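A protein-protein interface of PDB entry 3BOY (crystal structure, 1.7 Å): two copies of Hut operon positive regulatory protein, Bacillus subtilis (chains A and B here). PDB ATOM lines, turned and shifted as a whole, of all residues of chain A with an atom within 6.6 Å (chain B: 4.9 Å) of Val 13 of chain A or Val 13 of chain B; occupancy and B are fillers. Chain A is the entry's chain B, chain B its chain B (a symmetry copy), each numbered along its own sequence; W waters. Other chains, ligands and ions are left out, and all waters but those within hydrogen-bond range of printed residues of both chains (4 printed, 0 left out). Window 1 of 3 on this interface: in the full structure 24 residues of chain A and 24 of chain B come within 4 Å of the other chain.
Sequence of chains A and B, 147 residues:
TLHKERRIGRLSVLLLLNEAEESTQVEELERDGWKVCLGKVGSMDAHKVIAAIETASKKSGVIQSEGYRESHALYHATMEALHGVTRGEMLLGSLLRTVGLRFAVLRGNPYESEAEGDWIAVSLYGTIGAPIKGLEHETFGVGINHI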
ATOM      1  N   ILE A   8      23.575  34.807  17.361  1.00  0.00           N
ATOM      2  CA  ILE A   8      22.497  34.643  18.353  1.00  0.00           C
ATOM      3  C   ILE A   8      22.369  33.221  18.955  1.00  0.00           C
ATOM      4  O   ILE A   8      22.073  33.062  20.140  1.00  0.00           O
ATOM      5  CB  ILE A   8      21.148  35.110  17.747  1.00  0.00           C
ATOM      6  CG1 ILE A   8      20.053  35.234  18.828  1.00  0.00           C
ATOM      7  CG2 ILE A   8      20.725  34.162  16.556  1.00  0.00           C
ATOM      8  CD1 ILE A   8      18.727  35.730  18.267  1.00  0.00           C
ATOM      9  N   GLY A   9      22.613  32.206  18.124  1.00  0.00           N
ATOM     10  CA  GLY A   9      22.541  30.819  18.600  1.00  0.00           C
ATOM     11  C   GLY A   9      23.669  30.500  19.562  1.00  0.00           C
ATOM     12  O   GLY A   9      23.430  30.062  20.668  1.00  0.00           O
ATOM     13  N   ARG A  10      24.894  30.777  19.127  1.00  0.00           N
ATOM     14  CA  ARG A  10      26.078  30.544  19.955  1.00  0.00           C
ATOM     15  C   ARG A  10      26.045  31.356  21.256  1.00  0.00           C
ATOM     16  O   ARG A  10      26.331  30.829  22.320  1.00  0.00           O
ATOM     17  CB  ARG A  10      27.322  30.890  19.149  1.00  0.00           C
ATOM     18  CG  ARG A  10      28.589  30.844  19.970  1.00  0.00           C
ATOM     19  CD  ARG A  10      29.814  31.051  19.084  1.00  0.00           C
ATOM     20  NE  ARG A  10      31.039  30.940  19.877  1.00  0.00           N
ATOM     21  CZ  ARG A  10      31.622  31.949  20.521  1.00  0.00           C
ATOM     22  NH1 ARG A  10      31.103  33.182  20.480  1.00  0.00           N
ATOM     23  NH2 ARG A  10      32.733  31.722  21.212  1.00  0.00           N
ATOM     24  N   LEU A  11      25.654  32.624  21.159  1.00  0.00           N
ATOM     25  CA  LEU A  11      25.498  33.481  22.343  1.00  0.00           C
ATOM     26  C   LEU A  11      24.456  32.952  23.348  1.00  0.00           C
ATOM     27  O   LEU A  11      24.684  32.983  24.570  1.00  0.00           O
ATOM     28  CB  LEU A  11      25.215  34.939  21.948  1.00  0.00           C
ATOM     29  CG  LEU A  11      26.344  35.734  21.270  1.00  0.00           C
ATOM     30  CD1 LEU A  11      25.838  37.024  20.701  1.00  0.00           C
ATOM     31  CD2 LEU A  11      27.482  35.990  22.268  1.00  0.00           C
ATOM     32  N   SER A  12      23.317  32.471  22.848  1.00  0.00           N
ATOM     33  CA  SER A  12      22.270  31.947  23.739  1.00  0.00           C
ATOM     34  C   SER A  12      22.732  30.702  24.496  1.00  0.00           C
ATOM     35  O   SER A  12      22.410  30.535  25.679  1.00  0.00           O
ATOM     36  CB  SER A  12      20.953  31.701  22.987  1.00  0.00           C
ATOM     37  OG  SER A  12      21.036  30.600  22.111  1.00  0.00           O
ATOM     38  N   VAL A  13      23.533  29.869  23.819  1.00  0.00           N
ATOM     39  CA  VAL A  13      24.044  28.631  24.397  1.00  0.00           C
ATOM     40  C   VAL A  13      25.126  28.908  25.445  1.00  0.00           C
ATOM     41  O   VAL A  13      25.088  28.336  26.530  1.00  0.00           O
ATOM     42  CB  VAL A  13      24.542  27.666  23.279  1.00  0.00           C
ATOM     43  CG1 VAL A  13      25.244  26.444  23.855  1.00  0.00           C
ATOM     44  CG2 VAL A  13      23.330  27.198  22.441  1.00  0.00           C
ATOM     45  N   LEU A  14      26.050  29.807  25.120  1.00  0.00           N
ATOM     46  CA  LEU A  14      27.092  30.235  26.050  1.00  0.00           C
ATOM     47  C   LEU A  14      26.466  30.772  27.334  1.00  0.00           C
ATOM     48  O   LEU A  14      26.923  30.440  28.418  1.00  0.00           O
ATOM     49  CB  LEU A  14      28.021  31.282  25.415  1.00  0.00           C
ATOM     50  CG  LEU A  14      28.944  30.860  24.262  1.00  0.00           C
ATOM     51  CD2 LEU A  14      30.089  29.963  24.691  1.00  0.00           C
ATOM     52  N   LEU A  15      25.410  31.579  27.200  1.00  0.00           N
ATOM     53  CA  LEU A  15      24.665  32.120  28.351  1.00  0.00           C
ATOM     54  C   LEU A  15      24.113  30.981  29.186  1.00  0.00           C
ATOM     55  O   LEU A  15      24.272  30.950  30.409  1.00  0.00           O
ATOM     56  CB  LEU A  15      23.525  33.027  27.872  1.00  0.00           C
ATOM     57  CG  LEU A  15      22.698  33.794  28.921  1.00  0.00           C
ATOM     58  CD1 LEU A  15      23.560  34.749  29.761  1.00  0.00           C
ATOM     59  CD2 LEU A  15      21.565  34.529  28.226  1.00  0.00           C
ATOM     60  N   LEU A  16      23.491  30.014  28.518  1.00  0.00           N
ATOM     61  CA  LEU A  16      22.931  28.871  29.220  1.00  0.00           C
ATOM     62  C   LEU A  16      23.994  28.044  29.943  1.00  0.00           C
ATOM     63  O   LEU A  16      23.750  27.560  31.040  1.00  0.00           O
ATOM     64  CB  LEU A  16      22.103  27.997  28.260  1.00  0.00           C
ATOM     65  CG  LEU A  16      20.817  27.350  28.781  1.00  0.00           C
ATOM     66  CD1 LEU A  16      19.988  28.346  29.615  1.00  0.00           C
ATOM     67  N   LEU A  17      25.174  27.901  29.349  1.00  0.00           N
ATOM     68  CA  LEU A  17      26.152  26.928  29.846  1.00  0.00           C
ATOM     69  C   LEU A  17      27.114  27.458  30.899  1.00  0.00           C
ATOM     70  O   LEU A  17      27.835  26.687  31.530  1.00  0.00           O
ATOM     71  CB  LEU A  17      26.911  26.258  28.693  1.00  0.00           C
ATOM     72  CG  LEU A  17      26.066  25.320  27.823  1.00  0.00           C
ATOM     73  CD1 LEU A  17      26.955  24.617  26.809  1.00  0.00           C
ATOM     74  CD2 LEU A  17      25.278  24.305  28.648  1.00  0.00           C
ATOM     75  N   ASN A  18      27.113  28.770  31.087  1.00  0.00           N
ATOM     76  CA  ASN A  18      27.911  29.387  32.140  1.00  0.00           C
ATOM     77  C   ASN A  18      27.082  29.578  33.414  1.00  0.00           C
ATOM     78  O   ASN A  18      26.129  30.359  33.433  1.00  0.00           O
ATOM     79  CB  ASN A  18      28.510  30.712  31.650  1.00  0.00           C
ATOM     80  CG  ASN A  18      29.233  30.573  30.296  1.00  0.00           C
ATOM     81  OD1 ASN A  18      29.327  31.539  29.539  1.00  0.00           O
ATOM     82  ND2 ASN A  18      29.733  29.374  29.991  1.00  0.00           N
ATOM     83  N   ALA A 104      17.121  29.725  27.697  1.00  0.00           N
ATOM     84  CA  ALA A 104      17.466  31.100  27.379  1.00  0.00           C
ATOM     85  C   ALA A 104      16.699  31.505  26.113  1.00  0.00           C
ATOM     86  O   ALA A 104      16.586  30.714  25.174  1.00  0.00           O
ATOM     87  CB  ALA A 104      18.976  31.215  27.182  1.00  0.00           C
ATOM     88  N   LEU A 106      16.875  34.633  23.346  1.00  0.00           N
ATOM     89  CA  LEU A 106      17.605  35.832  22.885  1.00  0.00           C
ATOM     90  C   LEU A 106      16.916  36.396  21.677  1.00  0.00           C
ATOM     91  O   LEU A 106      16.488  35.646  20.800  1.00  0.00           O
ATOM     92  CB  LEU A 106      19.033  35.478  22.491  1.00  0.00           C
ATOM     93  CG  LEU A 106      20.183  35.827  23.415  1.00  0.00           C
ATOM     94  CD1 LEU A 106      20.111  34.906  24.626  1.00  0.00           C
ATOM     95  CD2 LEU A 106      21.505  35.655  22.661  1.00  0.00           C
ATOM     96  N   SER A 123      17.030  28.350  23.503  1.00  0.00           N
ATOM     97  CA  SER A 123      18.043  27.342  23.806  1.00  0.00           C
ATOM     98  C   SER A 123      17.687  26.632  25.076  1.00  0.00           C
ATOM     99  O   SER A 123      17.279  27.272  26.050  1.00  0.00           O
ATOM    100  CB  SER A 123      19.441  27.948  23.896  1.00  0.00           C
ATOM    101  OG  SER A 123      19.723  28.506  22.621  1.00  0.00           O
ATOM    102  N   LEU A 124      17.852  25.311  25.056  1.00  0.00           N
ATOM    103  CA  LEU A 124      17.493  24.453  26.189  1.00  0.00           C
ATOM    104  C   LEU A 124      18.628  23.516  26.548  1.00  0.00           C
ATOM    105  O   LEU A 124      19.269  22.941  25.660  1.00  0.00           O
ATOM    106  CB  LEU A 124      16.284  23.574  25.861  1.00  0.00           C
ATOM    107  CG  LEU A 124      15.117  24.272  25.188  1.00  0.00           C
ATOM    108  CD1 LEU A 124      14.096  23.247  24.684  1.00  0.00           C
ATOM    109  CD2 LEU A 124      14.422  25.218  26.182  1.00  0.00           C
ATOM    110  N   PHE A 140      19.920  18.778  24.978  1.00  0.00           N
ATOM    111  CA  PHE A 140      20.128  20.126  24.462  1.00  0.00           C
ATOM    112  C   PHE A 140      19.190  20.356  23.275  1.00  0.00           C
ATOM    113  O   PHE A 140      18.862  19.415  22.523  1.00  0.00           O
ATOM    114  CB  PHE A 140      21.510  20.303  23.789  1.00  0.00           C
ATOM    115  CG  PHE A 140      22.650  20.477  24.700  1.00  0.00           C
ATOM    116  CD1 PHE A 140      23.267  19.363  25.286  1.00  0.00           C
ATOM    117  CD2 PHE A 140      23.218  21.746  24.868  1.00  0.00           C
ATOM    118  CE1 PHE A 140      24.392  19.507  26.091  1.00  0.00           C
ATOM    119  CE2 PHE A 140      24.350  21.902  25.681  1.00  0.00           C
ATOM    120  CZ  PHE A 140      24.928  20.796  26.289  1.00  0.00           C
ATOM    121  N   GLY A 141      18.814  21.604  23.075  1.00  0.00           N
ATOM    122  CA  GLY A 141      18.065  21.973  21.871  1.00  0.00           C
ATOM    123  C   GLY A 141      18.205  23.447  21.604  1.00  0.00           C
ATOM    124  O   GLY A 141      18.256  24.244  22.529  1.00  0.00           O
ATOM    125  N   VAL A 142      18.303  23.794  20.331  1.00  0.00           N
ATOM    126  CA  VAL A 142      18.272  25.194  19.917  1.00  0.00           C
ATOM    127  C   VAL A 142      17.358  25.373  18.716  1.00  0.00           C
ATOM    128  O   VAL A 142      17.482  24.640  17.721  1.00  0.00           O
ATOM    129  CB  VAL A 142      19.697  25.649  19.516  1.00  0.00           C
ATOM    130  CG1 VAL A 142      19.682  27.119  19.016  1.00  0.00           C
ATOM    131  CG2 VAL A 142      20.606  25.517  20.732  1.00  0.00           C
ATOM    132  N   GLY B   9      28.047  16.148  27.967  1.00  0.00           N
ATOM    133  CA  GLY B   9      27.314  16.948  26.977  1.00  0.00           C
ATOM    134  C   GLY B   9      27.742  18.402  27.009  1.00  0.00           C
ATOM    135  O   GLY B   9      28.133  18.952  26.001  1.00  0.00           O
ATOM    136  N   ARG B  10      27.699  18.989  28.201  1.00  0.00           N
ATOM    137  CA  ARG B  10      28.105  20.383  28.390  1.00  0.00           C
ATOM    138  C   ARG B  10      29.571  20.618  28.005  1.00  0.00           C
ATOM    139  O   ARG B  10      29.884  21.582  27.324  1.00  0.00           O
ATOM    140  CB  ARG B  10      27.871  20.775  29.842  1.00  0.00           C
ATOM    141  CG  ARG B  10      28.415  22.144  30.179  1.00  0.00           C
ATOM    142  CD  ARG B  10      28.023  22.546  31.598  1.00  0.00           C
ATOM    143  NE  ARG B  10      28.498  23.898  31.892  1.00  0.00           N
ATOM    144  CZ  ARG B  10      29.698  24.192  32.389  1.00  0.00           C
ATOM    145  NH1 ARG B  10      30.583  23.226  32.663  1.00  0.00           N
ATOM    146  NH2 ARG B  10      30.016  25.461  32.611  1.00  0.00           N
ATOM    147  N   LEU B  11      30.448  19.706  28.414  1.00  0.00           N
ATOM    148  CA  LEU B  11      31.868  19.772  28.038  1.00  0.00           C
ATOM    149  C   LEU B  11      32.101  19.710  26.516  1.00  0.00           C
ATOM    150  O   LEU B  11      32.936  20.455  25.973  1.00  0.00           O
ATOM    151  CB  LEU B  11      32.696  18.712  28.781  1.00  0.00           C
ATOM    152  CG  LEU B  11      32.881  18.877  30.300  1.00  0.00           C
ATOM    153  CD1 LEU B  11      33.462  17.641  30.916  1.00  0.00           C
ATOM    154  CD2 LEU B  11      33.765  20.097  30.595  1.00  0.00           C
ATOM    155  N   SER B  12      31.377  18.830  25.823  1.00  0.00           N
ATOM    156  CA  SER B  12      31.538  18.707  24.366  1.00  0.00           C
ATOM    157  C   SER B  12      31.115  19.980  23.633  1.00  0.00           C
ATOM    158  O   SER B  12      31.758  20.382  22.656  1.00  0.00           O
ATOM    159  CB  SER B  12      30.819  17.466  23.816  1.00  0.00           C
ATOM    160  OG  SER B  12      29.417  17.603  23.848  1.00  0.00           O
ATOM    161  N   VAL B  13      30.066  20.632  24.152  1.00  0.00           N
ATOM    162  CA  VAL B  13      29.531  21.853  23.558  1.00  0.00           C
ATOM    163  C   VAL B  13      30.462  23.045  23.798  1.00  0.00           C
ATOM    164  O   VAL B  13      30.745  23.797  22.870  1.00  0.00           O
ATOM    165  CB  VAL B  13      28.084  22.124  24.069  1.00  0.00           C
ATOM    166  CG1 VAL B  13      27.565  23.480  23.611  1.00  0.00           C
ATOM    167  CG2 VAL B  13      27.144  21.021  23.532  1.00  0.00           C
ATOM    168  N   LEU B  14      30.951  23.179  25.027  1.00  0.00           N
ATOM    169  CA  LEU B  14      31.916  24.217  25.380  1.00  0.00           C
ATOM    170  C   LEU B  14      33.147  24.122  24.483  1.00  0.00           C
ATOM    171  O   LEU B  14      33.624  25.136  23.997  1.00  0.00           O
ATOM    172  CB  LEU B  14      32.313  24.138  26.863  1.00  0.00           C
ATOM    173  CG  LEU B  14      31.263  24.468  27.936  1.00  0.00           C
ATOM    174  CD2 LEU B  14      30.906  25.939  28.010  1.00  0.00           C
ATOM    175  N   LEU B  15      33.633  22.899  24.253  1.00  0.00           N
ATOM    176  CA  LEU B  15      34.777  22.649  23.357  1.00  0.00           C
ATOM    177  C   LEU B  15      34.453  23.148  21.963  1.00  0.00           C
ATOM    178  O   LEU B  15      35.240  23.870  21.344  1.00  0.00           O
ATOM    179  CB  LEU B  15      35.110  21.151  23.320  1.00  0.00           C
ATOM    180  CG  LEU B  15      36.353  20.688  22.537  1.00  0.00           C
ATOM    181  CD1 LEU B  15      37.650  21.311  23.077  1.00  0.00           C
ATOM    182  CD2 LEU B  15      36.414  19.171  22.546  1.00  0.00           C
ATOM    183  N   LEU B  16      33.268  22.795  21.474  1.00  0.00           N
ATOM    184  CA  LEU B  16      32.854  23.227  20.150  1.00  0.00           C
ATOM    185  C   LEU B  16      32.740  24.747  20.033  1.00  0.00           C
ATOM    186  O   LEU B  16      33.091  25.309  19.005  1.00  0.00           O
ATOM    187  CB  LEU B  16      31.540  22.537  19.739  1.00  0.00           C
ATOM    188  CG  LEU B  16      31.359  22.111  18.280  1.00  0.00           C
ATOM    189  CD1 LEU B  16      32.632  21.441  17.730  1.00  0.00           C
ATOM    190  N   LEU B  17      32.276  25.413  21.086  1.00  0.00           N
ATOM    191  CA  LEU B  17      31.901  26.826  20.973  1.00  0.00           C
ATOM    192  C   LEU B  17      33.021  27.817  21.252  1.00  0.00           C
ATOM    193  O   LEU B  17      32.879  29.010  20.991  1.00  0.00           O
ATOM    194  CB  LEU B  17      30.660  27.144  21.819  1.00  0.00           C
ATOM    195  CG  LEU B  17      29.357  26.513  21.315  1.00  0.00           C
ATOM    196  CD1 LEU B  17      28.187  27.011  22.148  1.00  0.00           C
ATOM    197  CD2 LEU B  17      29.113  26.775  19.830  1.00  0.00           C
ATOM    198  N   SER B 123      28.522  16.275  19.323  1.00  0.00           N
ATOM    199  CA  SER B 123      27.995  17.636  19.329  1.00  0.00           C
ATOM    200  C   SER B 123      28.286  18.299  18.019  1.00  0.00           C
ATOM    201  O   SER B 123      29.397  18.173  17.494  1.00  0.00           O
ATOM    202  CB  SER B 123      28.551  18.458  20.489  1.00  0.00           C
ATOM    203  OG  SER B 123      28.140  17.806  21.681  1.00  0.00           O
ATOM    204  N   PHE B 140      22.381  23.472  15.768  1.00  0.00           N
ATOM    205  CA  PHE B 140      23.062  22.773  16.852  1.00  0.00           C
ATOM    206  C   PHE B 140      22.425  21.393  17.032  1.00  0.00           C
ATOM    207  O   PHE B 140      21.213  21.209  16.799  1.00  0.00           O
ATOM    208  CB  PHE B 140      22.793  23.409  18.237  1.00  0.00           C
ATOM    209  CG  PHE B 140      23.557  24.625  18.544  1.00  0.00           C
ATOM    210  CD1 PHE B 140      23.123  25.874  18.076  1.00  0.00           C
ATOM    211  CD2 PHE B 140      24.639  24.561  19.431  1.00  0.00           C
ATOM    212  CE1 PHE B 140      23.795  27.042  18.419  1.00  0.00           C
ATOM    213  CE2 PHE B 140      25.325  25.733  19.781  1.00  0.00           C
ATOM    214  CZ  PHE B 140      24.911  26.959  19.278  1.00  0.00           C
ATOM    215  N   VAL B 142      23.046  17.761  19.806  1.00  0.00           N
ATOM    216  CA  VAL B 142      23.825  16.907  20.698  1.00  0.00           C
ATOM    217  C   VAL B 142      23.142  15.561  20.878  1.00  0.00           C
ATOM    218  O   VAL B 142      21.939  15.506  21.183  1.00  0.00           O
ATOM    219  CB  VAL B 142      23.946  17.581  22.087  1.00  0.00           C
ATOM    220  CG1 VAL B 142      24.721  16.666  23.074  1.00  0.00           C
ATOM    221  CG2 VAL B 142      24.674  18.908  21.918  1.00  0.00           C
HETATM  222  O   HOH W   1      19.430  21.421  18.819  1.00  0.00           O
HETATM  223  O   HOH W   2      19.948  16.282  22.985  1.00  0.00           O
HETATM  224  O   HOH W   3      19.193  23.659  15.740  1.00  0.00           O
HETATM  225  O   HOH W   4      20.299  18.950  20.282  1.00  0.00           O
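The backbone carbonyl oxygen of Leu 17 of chain B lies within hydrogen-bond range of the guanidinium group of Arg 10 of chain A (2.7 Å).
The backbone carbonyl oxygen (O) of Leu 17 of chain A is in hydrogen-bond range of the guanidinium group (NH2) of Arg 10 of chain B, 2.7 Å away.
The backbone carbonyl oxygen (O) of Gly 9 of chain A sits at hydrogen-bond distance from the side-chain hydroxyl (OG) of Ser 12 of chain A, 2.8 Å away.
OG of Ser 12 of chain B lies within hydrogen-bond range of O of Gly 9 of chain B (2.8 Å).
Among the printed residues, merely in contact across the chains: Gly 9 of chain A with Phe 140 of chain B (3.6 Å), Arg 10 of chain A with Phe 140 of chain B (3.8 Å), Val 13 of chain A with Val 13 of chain B (3.8 Å), Val 13 of chain A with Leu 17 of chain B (3.4 Å), Val 13 of chain A with Phe 140 of chain B (3.5 Å), Leu 17 of chain A with Val 13 of chain B (3.4 Å), Phe 140 of chain A with Gly 9 of chain B (3.6 Å), Phe 140 of chain A with Arg 10 of chain B (3.8 Å), Phe 140 of chain A with Val 13 of chain B (3.5 Å), Phe 140 of chain A with Val 142 of chain B (3.7 Å) and Val 142 of chain A with Phe 140 of chain B (3.7 Å).
Of chain B, only Val 13, Leu 17 and Phe 140 come within 4 Å of Val 13 of chain A.
Val 13 of chain B touches just these residues of chain A: Val 13 (3.8 Å), Leu 17 (3.4 Å) and Phe 140 (3.5 Å).
Of the printed residues of chain A, Arg 10 of chain B touches Leu 17 (2.7 Å) and Phe 140 (3.8 Å).
Printed residues of chain A within 4 Å of Gly 9 of chain B: Phe 140 (3.6 Å).
Of the printed residues of chain A, Val 142 of chain B touches Phe 140 (3.7 Å).
Of the printed residues of chain B, Gly 9 of chain A touches Phe 140.
The nearest printed residue of chain B that does not touch Val 13 of chain A is Leu 14 of chain B (6.5 Å).
The nearest printed residue of chain B that does not touch Phe 140 of chain A is Ser 12 of chain B (5.8 Å).
Hydrophobic or aromatic side chains of chain B within 4 Å of the printed part of chain A: Val 13, Leu 17, Phe 140 and Val 142.
Hydrophobic or aromatic side chains of chain A that line the printed part of chain B: Val 13, Leu 17, Phe 140 and Val 142.
Among the printed residues, no Asp or Glu carboxylate lies within 4 Å of a Lys or Arg side-chain nitrogen of the other chain.
Gly 9 of chain A touches Phe 140 of chain B, and with the chains exchanged Phe 140 of chain A touches Gly 9 of chain B.
Arg 10 of chain A touches Leu 17 of chain B, and with the chains exchanged Leu 17 of chain A touches Arg 10 of chain B.
Val 13 of chain A touches Leu 17 of chain B, and with the chains exchanged Leu 17 of chain A touches Val 13 of chain B.
Val 13 of chain A touches Phe 140 of chain B, and with the chains exchanged Phe 140 of chain A touches Val 13 of chain B.
Of the 13 pairs that touch across the chains among the printed residues, 13 have their exchanged pair printed and touching as well.
Water W4 lies within hydrogen-bond range of the backbone carbonyl oxygen of Phe 140 of chain A and the backbone NH of Val 142 of chain B.
Water W1 bridges O of Phe 140 of chain B and N of Val 142 of chain A.
Water W3 bridges the backbone carbonyl oxygen of Val 142 of chain A (2.8 Å) and the backbone NH of Phe 140 of chain B (3.2 Å).
Water W2 bridges the backbone carbonyl oxygen (O) of Val 142 of chain B and the backbone NH (N) of Phe 140 of chain A.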
